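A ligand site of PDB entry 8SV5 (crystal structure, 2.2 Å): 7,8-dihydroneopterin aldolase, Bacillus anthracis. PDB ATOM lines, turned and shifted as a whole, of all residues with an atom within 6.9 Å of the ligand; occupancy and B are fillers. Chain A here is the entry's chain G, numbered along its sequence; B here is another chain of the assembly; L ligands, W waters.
The side-chain carboxylate (OE2) of Glu 21 sits at hydrogen-bond distance from an oxygen (O2) of the ligand (2.7 Å).
An oxygen (O2) of the ligand sits at hydrogen-bond distance from the backbone NH (N) of Val 17 (2.8 Å).
The side-chain carboxylate (OE1) of Glu 73 is in hydrogen-bond range of a nitrogen (N5) of the ligand (2.8 Å).
The backbone carbonyl oxygen (O) of Val 51 of chain B lies within hydrogen-bond range of a nitrogen (N4) of the ligand, at 2.9 Å.
OD1 of Asn 52 of chain B lies within hydrogen-bond range of N2 of the ligand (2.9 Å).
An oxygen (O2) of the ligand sits at hydrogen-bond distance from the side-chain amino group (NZ) of Lys 99 (3.2 Å).
The backbone NH (N) of Val 72 is in hydrogen-bond range of an oxygen (O1) of the ligand, at 3.2 Å.
N of Tyr 53 of chain B lies within hydrogen-bond range of N3 of the ligand (3.2 Å).
OH of Tyr 53 of chain B sits close to N1 of the ligand (3.4 Å).
N4 of the ligand sits at hydrogen-bond distance from OG of Ser 50 of chain B (3.4 Å).
The side-chain carboxylate of Glu 21 lies within hydrogen-bond range of the backbone NH of Val 17, at 3.4 Å.
The side-chain amino group (NZ) of Lys 99 is in salt-bridge range of the side-chain carboxylate (OE1) of Glu 21 (2.9 Å).
The side-chain carboxylate (OE2) of Glu 21 lies close to the backbone NH (N) of Phe 18 (3.2 Å).
O of Lys 70 sits close to N of Val 17 (3.4 Å).
OD1 of Asn 52 of chain B sits at hydrogen-bond distance from N of Gly 54 of chain B (2.9 Å).
The side-chain amino group (NZ) of Lys 99 lies within hydrogen-bond range of the side-chain hydroxyl (OH) of Tyr 53 of chain B (2.8 Å).
The side-chain carboxylate (OD1) of Asp 45 of chain B is in hydrogen-bond range of the backbone NH (N) of Leu 71 (2.8 Å).
NZ of Lys 70 lies within hydrogen-bond range of O of Asp 45 of chain B, 2.6 Å away.
Residues that only touch the ligand: Gly 16 (3.5 Å), Phe 18 (3.9 Å), Lys 70 (3.8 Å), Leu 71 (3.3 Å), Ile 4 of chain B (3.9 Å) and Leu 47 of chain B (3.5 Å).
Hydrophobic or aromatic side chains within 4 Å of the ligand: Val 17, Phe 18, Leu 71, Val 72, Ile 4 of chain B, Leu 47 of chain B and Tyr 53 of chain B.
The nearest printed residue that does not touch the ligand is Gly 54 of chain B (4.4 Å).
Water W1 lies within hydrogen-bond range of an oxygen (O1) of the ligand (2.6 Å), the backbone carbonyl oxygen (O) of Lys 70 (2.9 Å) and the side-chain amino group (NZ) of Lys 99 (3.1 Å).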
ATOM      1  N   HIS A  15     -17.642 -12.835 -33.892  1.00  0.00           N
ATOM      2  CA  HIS A  15     -18.680 -13.706 -33.386  1.00  0.00           C
ATOM      3  C   HIS A  15     -18.973 -13.357 -31.927  1.00  0.00           C
ATOM      4  O   HIS A  15     -18.205 -12.659 -31.250  1.00  0.00           O
ATOM      5  CB  HIS A  15     -18.242 -15.163 -33.501  1.00  0.00           C
ATOM      6  CG  HIS A  15     -17.543 -15.492 -34.787  1.00  0.00           C
ATOM      7  ND1 HIS A  15     -18.182 -16.104 -35.843  1.00  0.00           N
ATOM      8  CD2 HIS A  15     -16.271 -15.282 -35.186  1.00  0.00           C
ATOM      9  CE1 HIS A  15     -17.330 -16.267 -36.835  1.00  0.00           C
ATOM     10  NE2 HIS A  15     -16.161 -15.772 -36.472  1.00  0.00           N
ATOM     11  N   GLY A  16     -20.113 -13.838 -31.445  1.00  0.00           N
ATOM     12  CA  GLY A  16     -20.548 -13.587 -30.084  1.00  0.00           C
ATOM     13  C   GLY A  16     -22.037 -13.289 -30.064  1.00  0.00           C
ATOM     14  O   GLY A  16     -22.618 -12.794 -31.034  1.00  0.00           O
ATOM     15  N   VAL A  17     -22.676 -13.598 -28.932  1.00  0.00           N
ATOM     16  CA  VAL A  17     -24.118 -13.370 -28.811  1.00  0.00           C
ATOM     17  C   VAL A  17     -24.452 -11.938 -28.424  1.00  0.00           C
ATOM     18  O   VAL A  17     -25.576 -11.488 -28.691  1.00  0.00           O
ATOM     19  CB  VAL A  17     -24.757 -14.385 -27.840  1.00  0.00           C
ATOM     20  CG1 VAL A  17     -24.241 -15.794 -28.123  1.00  0.00           C
ATOM     21  CG2 VAL A  17     -24.501 -13.998 -26.393  1.00  0.00           C
ATOM     22  N   PHE A  18     -23.523 -11.203 -27.821  1.00  0.00           N
ATOM     23  CA  PHE A  18     -23.789  -9.804 -27.487  1.00  0.00           C
ATOM     24  C   PHE A  18     -23.483  -8.916 -28.681  1.00  0.00           C
ATOM     25  O   PHE A  18     -22.402  -9.038 -29.277  1.00  0.00           O
ATOM     26  CB  PHE A  18     -22.920  -9.367 -26.309  1.00  0.00           C
ATOM     27  CG  PHE A  18     -23.093 -10.212 -25.068  1.00  0.00           C
ATOM     28  CD1 PHE A  18     -24.295 -10.221 -24.387  1.00  0.00           C
ATOM     29  CD2 PHE A  18     -22.043 -10.982 -24.596  1.00  0.00           C
ATOM     30  CE1 PHE A  18     -24.449 -10.993 -23.250  1.00  0.00           C
ATOM     31  CE2 PHE A  18     -22.198 -11.755 -23.459  1.00  0.00           C
ATOM     32  CZ  PHE A  18     -23.407 -11.755 -22.787  1.00  0.00           C
ATOM     33  N   GLU A  21     -20.047  -7.517 -28.982  1.00  0.00           N
ATOM     34  CA  GLU A  21     -18.977  -8.364 -29.517  1.00  0.00           C
ATOM     35  C   GLU A  21     -18.945  -8.298 -31.040  1.00  0.00           C
ATOM     36  O   GLU A  21     -17.867  -8.275 -31.638  1.00  0.00           O
ATOM     37  CB  GLU A  21     -19.187  -9.813 -29.068  1.00  0.00           C
ATOM     38  CG  GLU A  21     -19.135 -10.039 -27.566  1.00  0.00           C
ATOM     39  CD  GLU A  21     -19.378 -11.490 -27.208  1.00  0.00           C
ATOM     40  OE1 GLU A  21     -18.393 -12.268 -27.176  1.00  0.00           O
ATOM     41  OE2 GLU A  21     -20.548 -11.853 -26.976  1.00  0.00           O
ATOM     42  N   GLN A  26     -12.841  -9.836 -31.405  1.00  0.00           N
ATOM     43  CA  GLN A  26     -11.924 -10.338 -30.383  1.00  0.00           C
ATOM     44  C   GLN A  26     -11.104 -11.459 -31.010  1.00  0.00           C
ATOM     45  O   GLN A  26     -11.399 -11.921 -32.119  1.00  0.00           O
ATOM     46  CB  GLN A  26     -12.680 -10.850 -29.161  1.00  0.00           C
ATOM     47  CG  GLN A  26     -13.536 -12.084 -29.446  1.00  0.00           C
ATOM     48  CD  GLN A  26     -14.507 -12.387 -28.335  1.00  0.00           C
ATOM     49  OE1 GLN A  26     -14.122 -12.877 -27.267  1.00  0.00           O
ATOM     50  NE2 GLN A  26     -15.785 -12.101 -28.569  1.00  0.00           N
ATOM     51  N   LYS A  70     -23.284 -16.192 -33.901  1.00  0.00           N
ATOM     52  CA  LYS A  70     -23.452 -15.879 -32.490  1.00  0.00           C
ATOM     53  C   LYS A  70     -22.689 -16.857 -31.610  1.00  0.00           C
ATOM     54  O   LYS A  70     -22.118 -16.466 -30.578  1.00  0.00           O
ATOM     55  CB  LYS A  70     -24.936 -15.868 -32.125  1.00  0.00           C
ATOM     56  CG  LYS A  70     -25.688 -14.651 -32.650  1.00  0.00           C
ATOM     57  CD  LYS A  70     -27.083 -15.002 -33.134  1.00  0.00           C
ATOM     58  CE  LYS A  70     -27.963 -15.461 -31.988  1.00  0.00           C
ATOM     59  NZ  LYS A  70     -28.767 -16.660 -32.350  1.00  0.00           N
ATOM     60  N   LEU A  71     -22.651 -18.128 -32.008  1.00  0.00           N
ATOM     61  CA  LEU A  71     -22.065 -19.192 -31.194  1.00  0.00           C
ATOM     62  C   LEU A  71     -20.782 -19.709 -31.817  1.00  0.00           C
ATOM     63  O   LEU A  71     -20.695 -19.895 -33.035  1.00  0.00           O
ATOM     64  CB  LEU A  71     -23.046 -20.356 -31.061  1.00  0.00           C
ATOM     65  CG  LEU A  71     -24.460 -20.022 -30.603  1.00  0.00           C
ATOM     66  CD1 LEU A  71     -25.250 -21.301 -30.374  1.00  0.00           C
ATOM     67  CD2 LEU A  71     -24.431 -19.166 -29.344  1.00  0.00           C
ATOM     68  N   VAL A  72     -19.771 -19.936 -30.969  1.00  0.00           N
ATOM     69  CA  VAL A  72     -18.596 -20.681 -31.409  1.00  0.00           C
ATOM     70  C   VAL A  72     -18.989 -22.077 -31.843  1.00  0.00           C
ATOM     71  O   VAL A  72     -18.299 -22.706 -32.658  1.00  0.00           O
ATOM     72  CB  VAL A  72     -17.524 -20.702 -30.300  1.00  0.00           C
ATOM     73  CG1 VAL A  72     -16.846 -19.343 -30.185  1.00  0.00           C
ATOM     74  CG2 VAL A  72     -18.111 -21.134 -28.964  1.00  0.00           C
ATOM     75  N   GLU A  73     -20.101 -22.602 -31.323  1.00  0.00           N
ATOM     76  CA  GLU A  73     -20.642 -23.865 -31.815  1.00  0.00           C
ATOM     77  C   GLU A  73     -20.821 -23.829 -33.333  1.00  0.00           C
ATOM     78  O   GLU A  73     -20.530 -24.812 -34.022  1.00  0.00           O
ATOM     79  CB  GLU A  73     -21.990 -24.145 -31.146  1.00  0.00           C
ATOM     80  CG  GLU A  73     -21.885 -24.805 -29.786  1.00  0.00           C
ATOM     81  CD  GLU A  73     -21.910 -23.810 -28.645  1.00  0.00           C
ATOM     82  OE1 GLU A  73     -21.541 -22.632 -28.860  1.00  0.00           O
ATOM     83  OE2 GLU A  73     -22.288 -24.208 -27.516  1.00  0.00           O
ATOM     84  N   SER A  74     -21.297 -22.694 -33.865  1.00  0.00           N
ATOM     85  CA  SER A  74     -21.508 -22.590 -35.300  1.00  0.00           C
ATOM     86  C   SER A  74     -20.185 -22.574 -36.062  1.00  0.00           C
ATOM     87  O   SER A  74     -20.077 -23.162 -37.143  1.00  0.00           O
ATOM     88  CB  SER A  74     -22.328 -21.336 -35.616  1.00  0.00           C
ATOM     89  OG  SER A  74     -23.611 -21.418 -35.035  1.00  0.00           O
ATOM     90  N   LYS A  99     -12.164 -19.367 -27.415  1.00  0.00           N
ATOM     91  CA  LYS A  99     -12.381 -17.946 -27.171  1.00  0.00           C
ATOM     92  C   LYS A  99     -11.503 -17.559 -25.980  1.00  0.00           C
ATOM     93  O   LYS A  99     -11.879 -17.803 -24.827  1.00  0.00           O
ATOM     94  CB  LYS A  99     -13.859 -17.688 -26.852  1.00  0.00           C
ATOM     95  CG  LYS A  99     -14.436 -16.470 -27.532  1.00  0.00           C
ATOM     96  CD  LYS A  99     -15.955 -16.497 -27.521  1.00  0.00           C
ATOM     97  CE  LYS A  99     -16.530 -15.124 -27.272  1.00  0.00           C
ATOM     98  NZ  LYS A  99     -18.019 -15.148 -27.133  1.00  0.00           N
ATOM     99  N   PRO A 102     -13.163 -13.967 -23.581  1.00  0.00           N
ATOM    100  CA  PRO A 102     -14.616 -13.777 -23.560  1.00  0.00           C
ATOM    101  C   PRO A 102     -15.007 -12.664 -22.600  1.00  0.00           C
ATOM    102  O   PRO A 102     -14.213 -12.295 -21.718  1.00  0.00           O
ATOM    103  CB  PRO A 102     -15.141 -15.136 -23.085  1.00  0.00           C
ATOM    104  CG  PRO A 102     -14.039 -15.712 -22.289  1.00  0.00           C
ATOM    105  CD  PRO A 102     -12.755 -15.210 -22.904  1.00  0.00           C
ATOM    106  N   PRO A 103     -16.216 -12.124 -22.730  1.00  0.00           N
ATOM    107  CA  PRO A 103     -16.685 -11.092 -21.787  1.00  0.00           C
ATOM    108  C   PRO A 103     -17.279 -11.679 -20.518  1.00  0.00           C
ATOM    109  O   PRO A 103     -18.471 -11.517 -20.220  1.00  0.00           O
ATOM    110  CB  PRO A 103     -17.710 -10.328 -22.632  1.00  0.00           C
ATOM    111  CG  PRO A 103     -18.275 -11.368 -23.553  1.00  0.00           C
ATOM    112  CD  PRO A 103     -17.200 -12.401 -23.792  1.00  0.00           C
ATOM    113  N   ILE A 104     -16.460 -12.404 -19.754  1.00  0.00           N
ATOM    114  CA  ILE A 104     -16.871 -13.031 -18.526  1.00  0.00           C
ATOM    115  C   ILE A 104     -16.112 -12.370 -17.370  1.00  0.00           C
ATOM    116  O   ILE A 104     -14.886 -12.543 -17.270  1.00  0.00           O
ATOM    117  CB  ILE A 104     -16.607 -14.543 -18.531  1.00  0.00           C
ATOM    118  CG1 ILE A 104     -17.399 -15.219 -19.641  1.00  0.00           C
ATOM    119  CG2 ILE A 104     -16.958 -15.162 -17.182  1.00  0.00           C
ATOM    120  CD1 ILE A 104     -16.951 -16.625 -19.898  1.00  0.00           C
ATOM    121  N   VAL A 113     -15.193 -24.751 -27.299  1.00  0.00           N
ATOM    122  CA  VAL A 113     -16.072 -25.838 -27.695  1.00  0.00           C
ATOM    123  C   VAL A 113     -15.283 -26.765 -28.600  1.00  0.00           C
ATOM    124  O   VAL A 113     -14.469 -26.308 -29.416  1.00  0.00           O
ATOM    125  CB  VAL A 113     -17.352 -25.325 -28.407  1.00  0.00           C
ATOM    126  CG1 VAL A 113     -18.071 -24.322 -27.542  1.00  0.00           C
ATOM    127  CG2 VAL A 113     -17.001 -24.716 -29.754  1.00  0.00           C
ATOM    128  N   ILE B   4     -17.627 -28.717 -24.026  1.00  0.00           N
ATOM    129  CA  ILE B   4     -17.366 -27.324 -23.718  1.00  0.00           C
ATOM    130  C   ILE B   4     -16.297 -27.299 -22.629  1.00  0.00           C
ATOM    131  O   ILE B   4     -16.455 -27.953 -21.591  1.00  0.00           O
ATOM    132  CB  ILE B   4     -18.632 -26.584 -23.255  1.00  0.00           C
ATOM    133  CG1 ILE B   4     -19.554 -26.331 -24.451  1.00  0.00           C
ATOM    134  CG2 ILE B   4     -18.282 -25.260 -22.578  1.00  0.00           C
ATOM    135  CD1 ILE B   4     -20.968 -25.977 -24.066  1.00  0.00           C
ATOM    136  N   LEU B  38     -23.787 -30.741 -29.323  1.00  0.00           N
ATOM    137  CA  LEU B  38     -23.725 -29.363 -29.780  1.00  0.00           C
ATOM    138  C   LEU B  38     -24.118 -29.198 -31.246  1.00  0.00           C
ATOM    139  O   LEU B  38     -24.132 -28.077 -31.747  1.00  0.00           O
ATOM    140  CB  LEU B  38     -22.318 -28.795 -29.550  1.00  0.00           C
ATOM    141  CG  LEU B  38     -21.911 -28.637 -28.086  1.00  0.00           C
ATOM    142  CD1 LEU B  38     -20.492 -28.119 -27.985  1.00  0.00           C
ATOM    143  CD2 LEU B  38     -22.866 -27.712 -27.346  1.00  0.00           C
ATOM    144  N   ASP B  45     -27.344 -21.979 -34.508  1.00  0.00           N
ATOM    145  CA  ASP B  45     -26.738 -20.769 -33.961  1.00  0.00           C
ATOM    146  C   ASP B  45     -27.588 -20.180 -32.834  1.00  0.00           C
ATOM    147  O   ASP B  45     -27.632 -18.969 -32.641  1.00  0.00           O
ATOM    148  CB  ASP B  45     -26.474 -19.717 -35.037  1.00  0.00           C
ATOM    149  CG  ASP B  45     -25.328 -18.787 -34.693  1.00  0.00           C
ATOM    150  OD1 ASP B  45     -24.533 -19.123 -33.787  1.00  0.00           O
ATOM    151  OD2 ASP B  45     -25.220 -17.714 -35.319  1.00  0.00           O
ATOM    152  N   LEU B  47     -28.466 -20.255 -28.831  1.00  0.00           N
ATOM    153  CA  LEU B  47     -27.918 -20.654 -27.540  1.00  0.00           C
ATOM    154  C   LEU B  47     -28.870 -21.502 -26.713  1.00  0.00           C
ATOM    155  O   LEU B  47     -28.432 -22.201 -25.805  1.00  0.00           O
ATOM    156  CB  LEU B  47     -27.494 -19.418 -26.748  1.00  0.00           C
ATOM    157  CG  LEU B  47     -26.645 -19.626 -25.492  1.00  0.00           C
ATOM    158  CD1 LEU B  47     -25.406 -20.459 -25.784  1.00  0.00           C
ATOM    159  CD2 LEU B  47     -26.253 -18.286 -24.894  1.00  0.00           C
ATOM    160  N   SER B  50     -27.666 -25.047 -26.340  1.00  0.00           N
ATOM    161  CA  SER B  50     -26.405 -25.375 -25.683  1.00  0.00           C
ATOM    162  C   SER B  50     -26.466 -24.971 -24.210  1.00  0.00           C
ATOM    163  O   SER B  50     -27.542 -24.991 -23.598  1.00  0.00           O
ATOM    164  CB  SER B  50     -25.243 -24.688 -26.382  1.00  0.00           C
ATOM    165  OG  SER B  50     -23.998 -25.210 -25.928  1.00  0.00           O
ATOM    166  N   VAL B  51     -25.325 -24.620 -23.632  1.00  0.00           N
ATOM    167  CA  VAL B  51     -25.237 -24.194 -22.249  1.00  0.00           C
ATOM    168  C   VAL B  51     -24.353 -22.956 -22.193  1.00  0.00           C
ATOM    169  O   VAL B  51     -23.198 -22.997 -22.630  1.00  0.00           O
ATOM    170  CB  VAL B  51     -24.661 -25.305 -21.346  1.00  0.00           C
ATOM    171  CG1 VAL B  51     -24.522 -24.815 -19.907  1.00  0.00           C
ATOM    172  CG2 VAL B  51     -25.546 -26.543 -21.402  1.00  0.00           C
ATOM    173  N   ASN B  52     -24.895 -21.862 -21.671  1.00  0.00           N
ATOM    174  CA  ASN B  52     -24.152 -20.614 -21.557  1.00  0.00           C
ATOM    175  C   ASN B  52     -22.897 -20.837 -20.721  1.00  0.00           C
ATOM    176  O   ASN B  52     -22.988 -21.049 -19.504  1.00  0.00           O
ATOM    177  CB  ASN B  52     -25.034 -19.528 -20.926  1.00  0.00           C
ATOM    178  CG  ASN B  52     -24.396 -18.151 -20.979  1.00  0.00           C
ATOM    179  OD1 ASN B  52     -23.168 -18.015 -20.965  1.00  0.00           O
ATOM    180  ND2 ASN B  52     -25.228 -17.115 -21.040  1.00  0.00           N
ATOM    181  N   TYR B  53     -21.726 -20.789 -21.348  1.00  0.00           N
ATOM    182  CA  TYR B  53     -20.494 -21.074 -20.624  1.00  0.00           C
ATOM    183  C   TYR B  53     -20.239 -20.078 -19.493  1.00  0.00           C
ATOM    184  O   TYR B  53     -19.515 -20.395 -18.543  1.00  0.00           O
ATOM    185  CB  TYR B  53     -19.298 -21.168 -21.588  1.00  0.00           C
ATOM    186  CG  TYR B  53     -19.037 -19.953 -22.463  1.00  0.00           C
ATOM    187  CD1 TYR B  53     -18.962 -18.680 -21.913  1.00  0.00           C
ATOM    188  CD2 TYR B  53     -18.853 -20.085 -23.823  1.00  0.00           C
ATOM    189  CE1 TYR B  53     -18.728 -17.583 -22.700  1.00  0.00           C
ATOM    190  CE2 TYR B  53     -18.605 -18.984 -24.628  1.00  0.00           C
ATOM    191  CZ  TYR B  53     -18.537 -17.734 -24.048  1.00  0.00           C
ATOM    192  OH  TYR B  53     -18.296 -16.610 -24.814  1.00  0.00           O
ATOM    193  N   GLY B  54     -20.828 -18.873 -19.573  1.00  0.00           N
ATOM    194  CA  GLY B  54     -20.650 -17.908 -18.502  1.00  0.00           C
ATOM    195  C   GLY B  54     -21.349 -18.324 -17.219  1.00  0.00           C
ATOM    196  O   GLY B  54     -20.875 -18.019 -16.125  1.00  0.00           O
ATOM    197  N   GLU B  55     -22.484 -19.003 -17.344  1.00  0.00           N
ATOM    198  CA  GLU B  55     -23.142 -19.547 -16.165  1.00  0.00           C
ATOM    199  C   GLU B  55     -22.343 -20.704 -15.561  1.00  0.00           C
ATOM    200  O   GLU B  55     -22.369 -20.913 -14.348  1.00  0.00           O
ATOM    201  CB  GLU B  55     -24.544 -20.026 -16.517  1.00  0.00           C
ATOM    202  CG  GLU B  55     -25.543 -18.896 -16.740  1.00  0.00           C
ATOM    203  CD  GLU B  55     -26.759 -19.351 -17.523  1.00  0.00           C
ATOM    204  OE1 GLU B  55     -27.045 -20.561 -17.535  1.00  0.00           O
ATOM    205  OE2 GLU B  55     -27.432 -18.481 -18.135  1.00  0.00           O
HETATM  206  N1  LIG L   1     -21.326 -17.188 -26.157  1.00  0.00           N
HETATM  207  C1  LIG L   1     -21.553 -16.330 -25.228  1.00  0.00           C
HETATM  208  C2  LIG L   1     -22.362 -16.685 -24.025  1.00  0.00           C
HETATM  209  N2  LIG L   1     -22.156 -18.099 -23.676  1.00  0.00           N
HETATM  210  N3  LIG L   1     -22.110 -20.286 -24.521  1.00  0.00           N
HETATM  211  C3  LIG L   1     -21.888 -21.146 -25.493  1.00  0.00           C
HETATM  212  N4  LIG L   1     -22.086 -22.478 -25.249  1.00  0.00           N
HETATM  213  N5  LIG L   1     -21.486 -20.748 -26.723  1.00  0.00           N
HETATM  214  C4  LIG L   1     -21.286 -19.442 -26.982  1.00  0.00           C
HETATM  215  O1  LIG L   1     -20.916 -19.085 -28.077  1.00  0.00           O
HETATM  216  C5  LIG L   1     -21.521 -18.512 -25.953  1.00  0.00           C
HETATM  217  C6  LIG L   1     -21.937 -18.986 -24.707  1.00  0.00           C
HETATM  218  C7  LIG L   1     -21.057 -14.912 -25.366  1.00  0.00           C
HETATM  219  O2  LIG L   1     -21.112 -14.512 -26.737  1.00  0.00           O
HETATM  220  O   HOH W   1     -19.678 -16.950 -29.024  1.00  0.00           O
